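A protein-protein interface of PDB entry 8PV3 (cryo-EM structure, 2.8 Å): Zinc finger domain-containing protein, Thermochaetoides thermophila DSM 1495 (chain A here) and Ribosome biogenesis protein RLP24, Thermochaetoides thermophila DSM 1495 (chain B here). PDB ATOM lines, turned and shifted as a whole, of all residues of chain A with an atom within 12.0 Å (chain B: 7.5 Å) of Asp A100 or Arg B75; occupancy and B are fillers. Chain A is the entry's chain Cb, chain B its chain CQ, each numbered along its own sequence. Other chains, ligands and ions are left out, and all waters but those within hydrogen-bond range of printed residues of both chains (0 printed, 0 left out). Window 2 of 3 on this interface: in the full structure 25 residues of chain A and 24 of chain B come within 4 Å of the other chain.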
ATOM      1  N   GLU A  89       5.249 -35.230   7.412  1.00  0.00           N
ATOM      2  CA  GLU A  89       3.868 -35.575   7.085  1.00  0.00           C
ATOM      3  C   GLU A  89       3.549 -37.008   7.491  1.00  0.00           C
ATOM      4  O   GLU A  89       2.479 -37.278   8.049  1.00  0.00           O
ATOM      5  CB  GLU A  89       3.610 -35.369   5.593  1.00  0.00           C
ATOM      6  CG  GLU A  89       3.624 -33.915   5.151  1.00  0.00           C
ATOM      7  CD  GLU A  89       5.008 -33.429   4.772  1.00  0.00           C
ATOM      8  OE1 GLU A  89       5.950 -34.249   4.775  1.00  0.00           O
ATOM      9  OE2 GLU A  89       5.156 -32.226   4.472  1.00  0.00           O
ATOM     10  N   MET A  92       3.250 -37.050  11.293  1.00  0.00           N
ATOM     11  CA  MET A  92       1.938 -36.615  11.764  1.00  0.00           C
ATOM     12  C   MET A  92       0.869 -37.664  11.478  1.00  0.00           C
ATOM     13  O   MET A  92      -0.026 -37.887  12.302  1.00  0.00           O
ATOM     14  CB  MET A  92       1.554 -35.279  11.130  1.00  0.00           C
ATOM     15  CG  MET A  92       2.419 -34.108  11.551  1.00  0.00           C
ATOM     16  SD  MET A  92       1.865 -32.558  10.817  1.00  0.00           S
ATOM     17  CE  MET A  92       2.411 -32.764   9.126  1.00  0.00           C
ATOM     18  N   GLY A  96      -1.921 -39.570  13.762  1.00  0.00           N
ATOM     19  CA  GLY A  96      -3.220 -39.030  13.411  1.00  0.00           C
ATOM     20  C   GLY A  96      -3.316 -37.532  13.568  1.00  0.00           C
ATOM     21  O   GLY A  96      -4.396 -37.011  13.858  1.00  0.00           O
ATOM     22  N   TYR A  97      -2.207 -36.825  13.385  1.00  0.00           N
ATOM     23  CA  TYR A  97      -2.140 -35.385  13.553  1.00  0.00           C
ATOM     24  C   TYR A  97      -2.250 -34.702  12.197  1.00  0.00           C
ATOM     25  O   TYR A  97      -1.772 -35.219  11.183  1.00  0.00           O
ATOM     26  CB  TYR A  97      -0.831 -34.984  14.240  1.00  0.00           C
ATOM     27  CG  TYR A  97      -0.862 -33.638  14.924  1.00  0.00           C
ATOM     28  CD1 TYR A  97      -1.799 -33.360  15.908  1.00  0.00           C
ATOM     29  CD2 TYR A  97       0.060 -32.653  14.598  1.00  0.00           C
ATOM     30  CE1 TYR A  97      -1.825 -32.133  16.540  1.00  0.00           C
ATOM     31  CE2 TYR A  97       0.043 -31.425  15.225  1.00  0.00           C
ATOM     32  CZ  TYR A  97      -0.901 -31.171  16.194  1.00  0.00           C
ATOM     33  OH  TYR A  97      -0.922 -29.946  16.822  1.00  0.00           O
ATOM     34  N   ARG A  98      -2.893 -33.539  12.182  1.00  0.00           N
ATOM     35  CA  ARG A  98      -3.043 -32.758  10.965  1.00  0.00           C
ATOM     36  C   ARG A  98      -2.703 -31.308  11.268  1.00  0.00           C
ATOM     37  O   ARG A  98      -2.433 -30.932  12.411  1.00  0.00           O
ATOM     38  CB  ARG A  98      -4.460 -32.856  10.393  1.00  0.00           C
ATOM     39  CG  ARG A  98      -5.504 -32.240  11.291  1.00  0.00           C
ATOM     40  CD  ARG A  98      -6.907 -32.390  10.745  1.00  0.00           C
ATOM     41  NE  ARG A  98      -7.882 -31.778  11.638  1.00  0.00           N
ATOM     42  CZ  ARG A  98      -9.188 -31.737  11.414  1.00  0.00           C
ATOM     43  NH1 ARG A  98      -9.718 -32.266  10.323  1.00  0.00           N
ATOM     44  NH2 ARG A  98      -9.980 -31.149  12.304  1.00  0.00           N
ATOM     45  N   ILE A  99      -2.719 -30.487  10.221  1.00  0.00           N
ATOM     46  CA  ILE A  99      -2.468 -29.057  10.329  1.00  0.00           C
ATOM     47  C   ILE A  99      -3.722 -28.329   9.869  1.00  0.00           C
ATOM     48  O   ILE A  99      -4.219 -28.572   8.763  1.00  0.00           O
ATOM     49  CB  ILE A  99      -1.244 -28.632   9.504  1.00  0.00           C
ATOM     50  CG1 ILE A  99       0.018 -29.309  10.038  1.00  0.00           C
ATOM     51  CG2 ILE A  99      -1.081 -27.125   9.520  1.00  0.00           C
ATOM     52  CD1 ILE A  99       1.218 -29.152   9.134  1.00  0.00           C
ATOM     53  N   ASP A 100      -4.238 -27.445  10.717  1.00  0.00           N
ATOM     54  CA  ASP A 100      -5.425 -26.661  10.409  1.00  0.00           C
ATOM     55  C   ASP A 100      -4.989 -25.260   9.995  1.00  0.00           C
ATOM     56  O   ASP A 100      -4.396 -24.528  10.794  1.00  0.00           O
ATOM     57  CB  ASP A 100      -6.363 -26.605  11.616  1.00  0.00           C
ATOM     58  CG  ASP A 100      -7.652 -25.861  11.324  1.00  0.00           C
ATOM     59  OD1 ASP A 100      -8.029 -25.750  10.138  1.00  0.00           O
ATOM     60  OD2 ASP A 100      -8.289 -25.384  12.285  1.00  0.00           O
ATOM     61  N   ASN A 101      -5.284 -24.895   8.748  1.00  0.00           N
ATOM     62  CA  ASN A 101      -4.906 -23.600   8.198  1.00  0.00           C
ATOM     63  C   ASN A 101      -6.117 -22.740   7.859  1.00  0.00           C
ATOM     64  O   ASN A 101      -6.009 -21.811   7.053  1.00  0.00           O
ATOM     65  CB  ASN A 101      -4.028 -23.789   6.961  1.00  0.00           C
ATOM     66  CG  ASN A 101      -2.644 -24.301   7.302  1.00  0.00           C
ATOM     67  OD1 ASN A 101      -2.121 -24.034   8.382  1.00  0.00           O
ATOM     68  ND2 ASN A 101      -2.043 -25.042   6.380  1.00  0.00           N
ATOM     69  N   GLY A 102      -7.269 -23.032   8.454  1.00  0.00           N
ATOM     70  CA  GLY A 102      -8.476 -22.272   8.190  1.00  0.00           C
ATOM     71  C   GLY A 102      -9.094 -22.576   6.840  1.00  0.00           C
ATOM     72  O   GLY A 102     -10.313 -22.530   6.680  1.00  0.00           O
ATOM     73  N   ARG B   2       3.768 -26.664  25.726  1.00  0.00           N
ATOM     74  CA  ARG B   2       2.912 -27.591  25.005  1.00  0.00           C
ATOM     75  C   ARG B   2       3.588 -28.951  24.950  1.00  0.00           C
ATOM     76  O   ARG B   2       4.729 -29.119  25.385  1.00  0.00           O
ATOM     77  CB  ARG B   2       2.606 -27.084  23.591  1.00  0.00           C
ATOM     78  CG  ARG B   2       3.809 -27.089  22.669  1.00  0.00           C
ATOM     79  CD  ARG B   2       3.424 -26.809  21.228  1.00  0.00           C
ATOM     80  NE  ARG B   2       2.773 -27.943  20.587  1.00  0.00           N
ATOM     81  CZ  ARG B   2       1.475 -28.017  20.334  1.00  0.00           C
ATOM     82  NH1 ARG B   2       0.650 -27.037  20.663  1.00  0.00           N
ATOM     83  NH2 ARG B   2       0.992 -29.099  19.729  1.00  0.00           N
ATOM     84  N   GLN B  70     -10.495 -36.261  14.367  1.00  0.00           N
ATOM     85  CA  GLN B  70     -10.564 -35.003  13.640  1.00  0.00           C
ATOM     86  C   GLN B  70     -10.669 -33.793  14.556  1.00  0.00           C
ATOM     87  O   GLN B  70     -10.714 -32.662  14.063  1.00  0.00           O
ATOM     88  CB  GLN B  70     -11.756 -35.022  12.678  1.00  0.00           C
ATOM     89  CG  GLN B  70     -11.654 -36.071  11.588  1.00  0.00           C
ATOM     90  CD  GLN B  70     -10.519 -35.798  10.625  1.00  0.00           C
ATOM     91  OE1 GLN B  70     -10.257 -34.650  10.268  1.00  0.00           O
ATOM     92  NE2 GLN B  70      -9.839 -36.855  10.195  1.00  0.00           N
ATOM     93  N   PHE B  71     -10.709 -34.000  15.869  1.00  0.00           N
ATOM     94  CA  PHE B  71     -10.872 -32.902  16.810  1.00  0.00           C
ATOM     95  C   PHE B  71      -9.554 -32.297  17.269  1.00  0.00           C
ATOM     96  O   PHE B  71      -9.558 -31.189  17.814  1.00  0.00           O
ATOM     97  CB  PHE B  71     -11.662 -33.374  18.032  1.00  0.00           C
ATOM     98  CG  PHE B  71     -13.101 -33.679  17.740  1.00  0.00           C
ATOM     99  CD1 PHE B  71     -14.061 -32.685  17.827  1.00  0.00           C
ATOM    100  CD2 PHE B  71     -13.498 -34.960  17.396  1.00  0.00           C
ATOM    101  CE1 PHE B  71     -15.387 -32.960  17.566  1.00  0.00           C
ATOM    102  CE2 PHE B  71     -14.824 -35.240  17.133  1.00  0.00           C
ATOM    103  CZ  PHE B  71     -15.770 -34.239  17.218  1.00  0.00           C
ATOM    104  N   ALA B  72      -8.437 -32.986  17.065  1.00  0.00           N
ATOM    105  CA  ALA B  72      -7.119 -32.477  17.417  1.00  0.00           C
ATOM    106  C   ALA B  72      -6.381 -32.092  16.145  1.00  0.00           C
ATOM    107  O   ALA B  72      -6.282 -32.895  15.212  1.00  0.00           O
ATOM    108  CB  ALA B  72      -6.318 -33.514  18.204  1.00  0.00           C
ATOM    109  N   ALA B  73      -5.864 -30.867  16.113  1.00  0.00           N
ATOM    110  CA  ALA B  73      -5.183 -30.352  14.938  1.00  0.00           C
ATOM    111  C   ALA B  73      -4.208 -29.271  15.369  1.00  0.00           C
ATOM    112  O   ALA B  73      -4.297 -28.734  16.474  1.00  0.00           O
ATOM    113  CB  ALA B  73      -6.176 -29.791  13.916  1.00  0.00           C
ATOM    114  N   ARG B  74      -3.267 -28.957  14.485  1.00  0.00           N
ATOM    115  CA  ARG B  74      -2.403 -27.802  14.689  1.00  0.00           C
ATOM    116  C   ARG B  74      -3.144 -26.572  14.186  1.00  0.00           C
ATOM    117  O   ARG B  74      -3.314 -26.388  12.978  1.00  0.00           O
ATOM    118  CB  ARG B  74      -1.070 -27.987  13.973  1.00  0.00           C
ATOM    119  CG  ARG B  74      -0.202 -26.743  13.958  1.00  0.00           C
ATOM    120  CD  ARG B  74       1.083 -26.977  13.175  1.00  0.00           C
ATOM    121  NE  ARG B  74       2.042 -25.884  13.294  1.00  0.00           N
ATOM    122  CZ  ARG B  74       2.719 -25.569  14.393  1.00  0.00           C
ATOM    123  NH1 ARG B  74       2.612 -26.279  15.504  1.00  0.00           N
ATOM    124  NH2 ARG B  74       3.540 -24.524  14.368  1.00  0.00           N
ATOM    125  N   ARG B  75      -3.600 -25.737  15.113  1.00  0.00           N
ATOM    126  CA  ARG B  75      -4.445 -24.595  14.788  1.00  0.00           C
ATOM    127  C   ARG B  75      -3.552 -23.402  14.472  1.00  0.00           C
ATOM    128  O   ARG B  75      -2.980 -22.787  15.377  1.00  0.00           O
ATOM    129  CB  ARG B  75      -5.392 -24.288  15.944  1.00  0.00           C
ATOM    130  CG  ARG B  75      -6.058 -25.519  16.528  1.00  0.00           C
ATOM    131  CD  ARG B  75      -7.184 -26.012  15.643  1.00  0.00           C
ATOM    132  NE  ARG B  75      -7.733 -27.278  16.113  1.00  0.00           N
ATOM    133  CZ  ARG B  75      -8.847 -27.826  15.652  1.00  0.00           C
ATOM    134  NH1 ARG B  75      -9.572 -27.237  14.716  1.00  0.00           N
ATOM    135  NH2 ARG B  75      -9.248 -28.993  16.145  1.00  0.00           N
ATOM    136  N   ASN B  76      -3.434 -23.076  13.188  1.00  0.00           N
ATOM    137  CA  ASN B  76      -2.618 -21.958  12.746  1.00  0.00           C
ATOM    138  C   ASN B  76      -3.381 -20.643  12.704  1.00  0.00           C
ATOM    139  O   ASN B  76      -2.764 -19.593  12.506  1.00  0.00           O
ATOM    140  CB  ASN B  76      -2.028 -22.252  11.364  1.00  0.00           C
ATOM    141  CG  ASN B  76      -0.867 -23.220  11.423  1.00  0.00           C
ATOM    142  OD1 ASN B  76      -0.242 -23.394  12.466  1.00  0.00           O
ATOM    143  ND2 ASN B  76      -0.570 -23.853  10.299  1.00  0.00           N
ATOM    144  N   VAL B  77      -4.697 -20.675  12.885  1.00  0.00           N
ATOM    145  CA  VAL B  77      -5.498 -19.459  12.981  1.00  0.00           C
ATOM    146  C   VAL B  77      -5.957 -19.314  14.426  1.00  0.00           C
ATOM    147  O   VAL B  77      -6.776 -20.117  14.896  1.00  0.00           O
ATOM    148  CB  VAL B  77      -6.688 -19.493  12.011  1.00  0.00           C
ATOM    149  CG1 VAL B  77      -7.491 -18.212  12.120  1.00  0.00           C
ATOM    150  CG2 VAL B  77      -6.199 -19.696  10.591  1.00  0.00           C
ATOM    151  N   PRO B  78      -5.446 -18.332  15.167  1.00  0.00           N
ATOM    152  CA  PRO B  78      -5.812 -18.205  16.582  1.00  0.00           C
ATOM    153  C   PRO B  78      -7.252 -17.753  16.767  1.00  0.00           C
ATOM    154  O   PRO B  78      -7.834 -17.076  15.917  1.00  0.00           O
ATOM    155  CB  PRO B  78      -4.830 -17.154  17.104  1.00  0.00           C
ATOM    156  CG  PRO B  78      -4.490 -16.349  15.905  1.00  0.00           C
ATOM    157  CD  PRO B  78      -4.453 -17.323  14.768  1.00  0.00           C
ATOM    158  N   VAL B  79      -7.822 -18.145  17.901  1.00  0.00           N
ATOM    159  CA  VAL B  79      -9.173 -17.770  18.294  1.00  0.00           C
ATOM    160  C   VAL B  79      -9.076 -16.845  19.500  1.00  0.00           C
ATOM    161  O   VAL B  79      -8.270 -17.084  20.407  1.00  0.00           O
ATOM    162  CB  VAL B  79     -10.021 -19.020  18.605  1.00  0.00           C
ATOM    163  CG1 VAL B  79     -11.410 -18.643  19.090  1.00  0.00           C
ATOM    164  CG2 VAL B  79     -10.106 -19.914  17.383  1.00  0.00           C
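Hydrophobic or aromatic side chains of chain A that line the printed part of chain B: Tyr A97 and Ile A99.
The backbone NH of Arg B74 lies within hydrogen-bond range of the backbone carbonyl oxygen of Arg A98 (3.0 Å). N of Arg B74 lies close to OH of Tyr A97 (3.5 Å). NH1 of Arg B75 is in salt-bridge range of OD2 of Asp A100 (3.3 Å). ND2 of Asn B76 is in hydrogen-bond range of OD1 of Asn A101, 2.5 Å away. The backbone carbonyl oxygen of Arg B74 sits at hydrogen-bond distance from the backbone NH of Asp A100 (2.7 Å). The backbone carbonyl oxygen of Gln B70 is in hydrogen-bond range of the guanidinium group of Arg A98, at 2.4 Å. The backbone NH of Asn B76 is in hydrogen-bond range of the backbone carbonyl oxygen of Asp A100 (3.0 Å).
Of the printed residues of chain B, Ile A99 touches Arg B74 and Asn B76. Printed residues of chain A within 4 Å of Arg B2: Tyr A97. Phe B71 touches none of the printed residues of chain A. Of chain A, only Tyr A97 (3.6 Å), Arg A98 (3.5 Å) and Asp A100 (3.9 Å) come within 4 Å of Ala B73. Arg B74 touches just these residues of chain A: Tyr A97 (3.4 Å), Arg A98 (3.0 Å), Ile A99 (3.7 Å) and Asp A100 (2.7 Å). Arg B75 touches just one residue of chain A: Asp A100. Asn B76 touches three residues of chain A. No residue of chain A comes within 4 Å of Val B77. The nearest residue of chain A that does not touch Arg B75 is Arg A98 (4.5 Å).
NH2 of Arg B75 lies within hydrogen-bond range of O of Phe B71 (2.8 Å). The backbone carbonyl oxygen (O) of Met A92 sits at hydrogen-bond distance from the backbone NH (N) of Tyr A97. The side-chain amide oxygen of Asn B76 is in hydrogen-bond range of the guanidinium group of Arg B74, at 3.5 Å. The backbone NH (N) of Gly A102 sits at hydrogen-bond distance from the side-chain carboxylate (OD1) of Asp A100 (3.3 Å).
OH of Tyr A97 touches NH2 of Arg B2, at 3.6 Å. Tyr A97 touches Ala B73 (OH to O, 3.6 Å). Ala B73 touches Arg A98. Ile A99 touches Arg B74. Asn B76 touches Ile A99. Ala B73 touches Asp A100.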
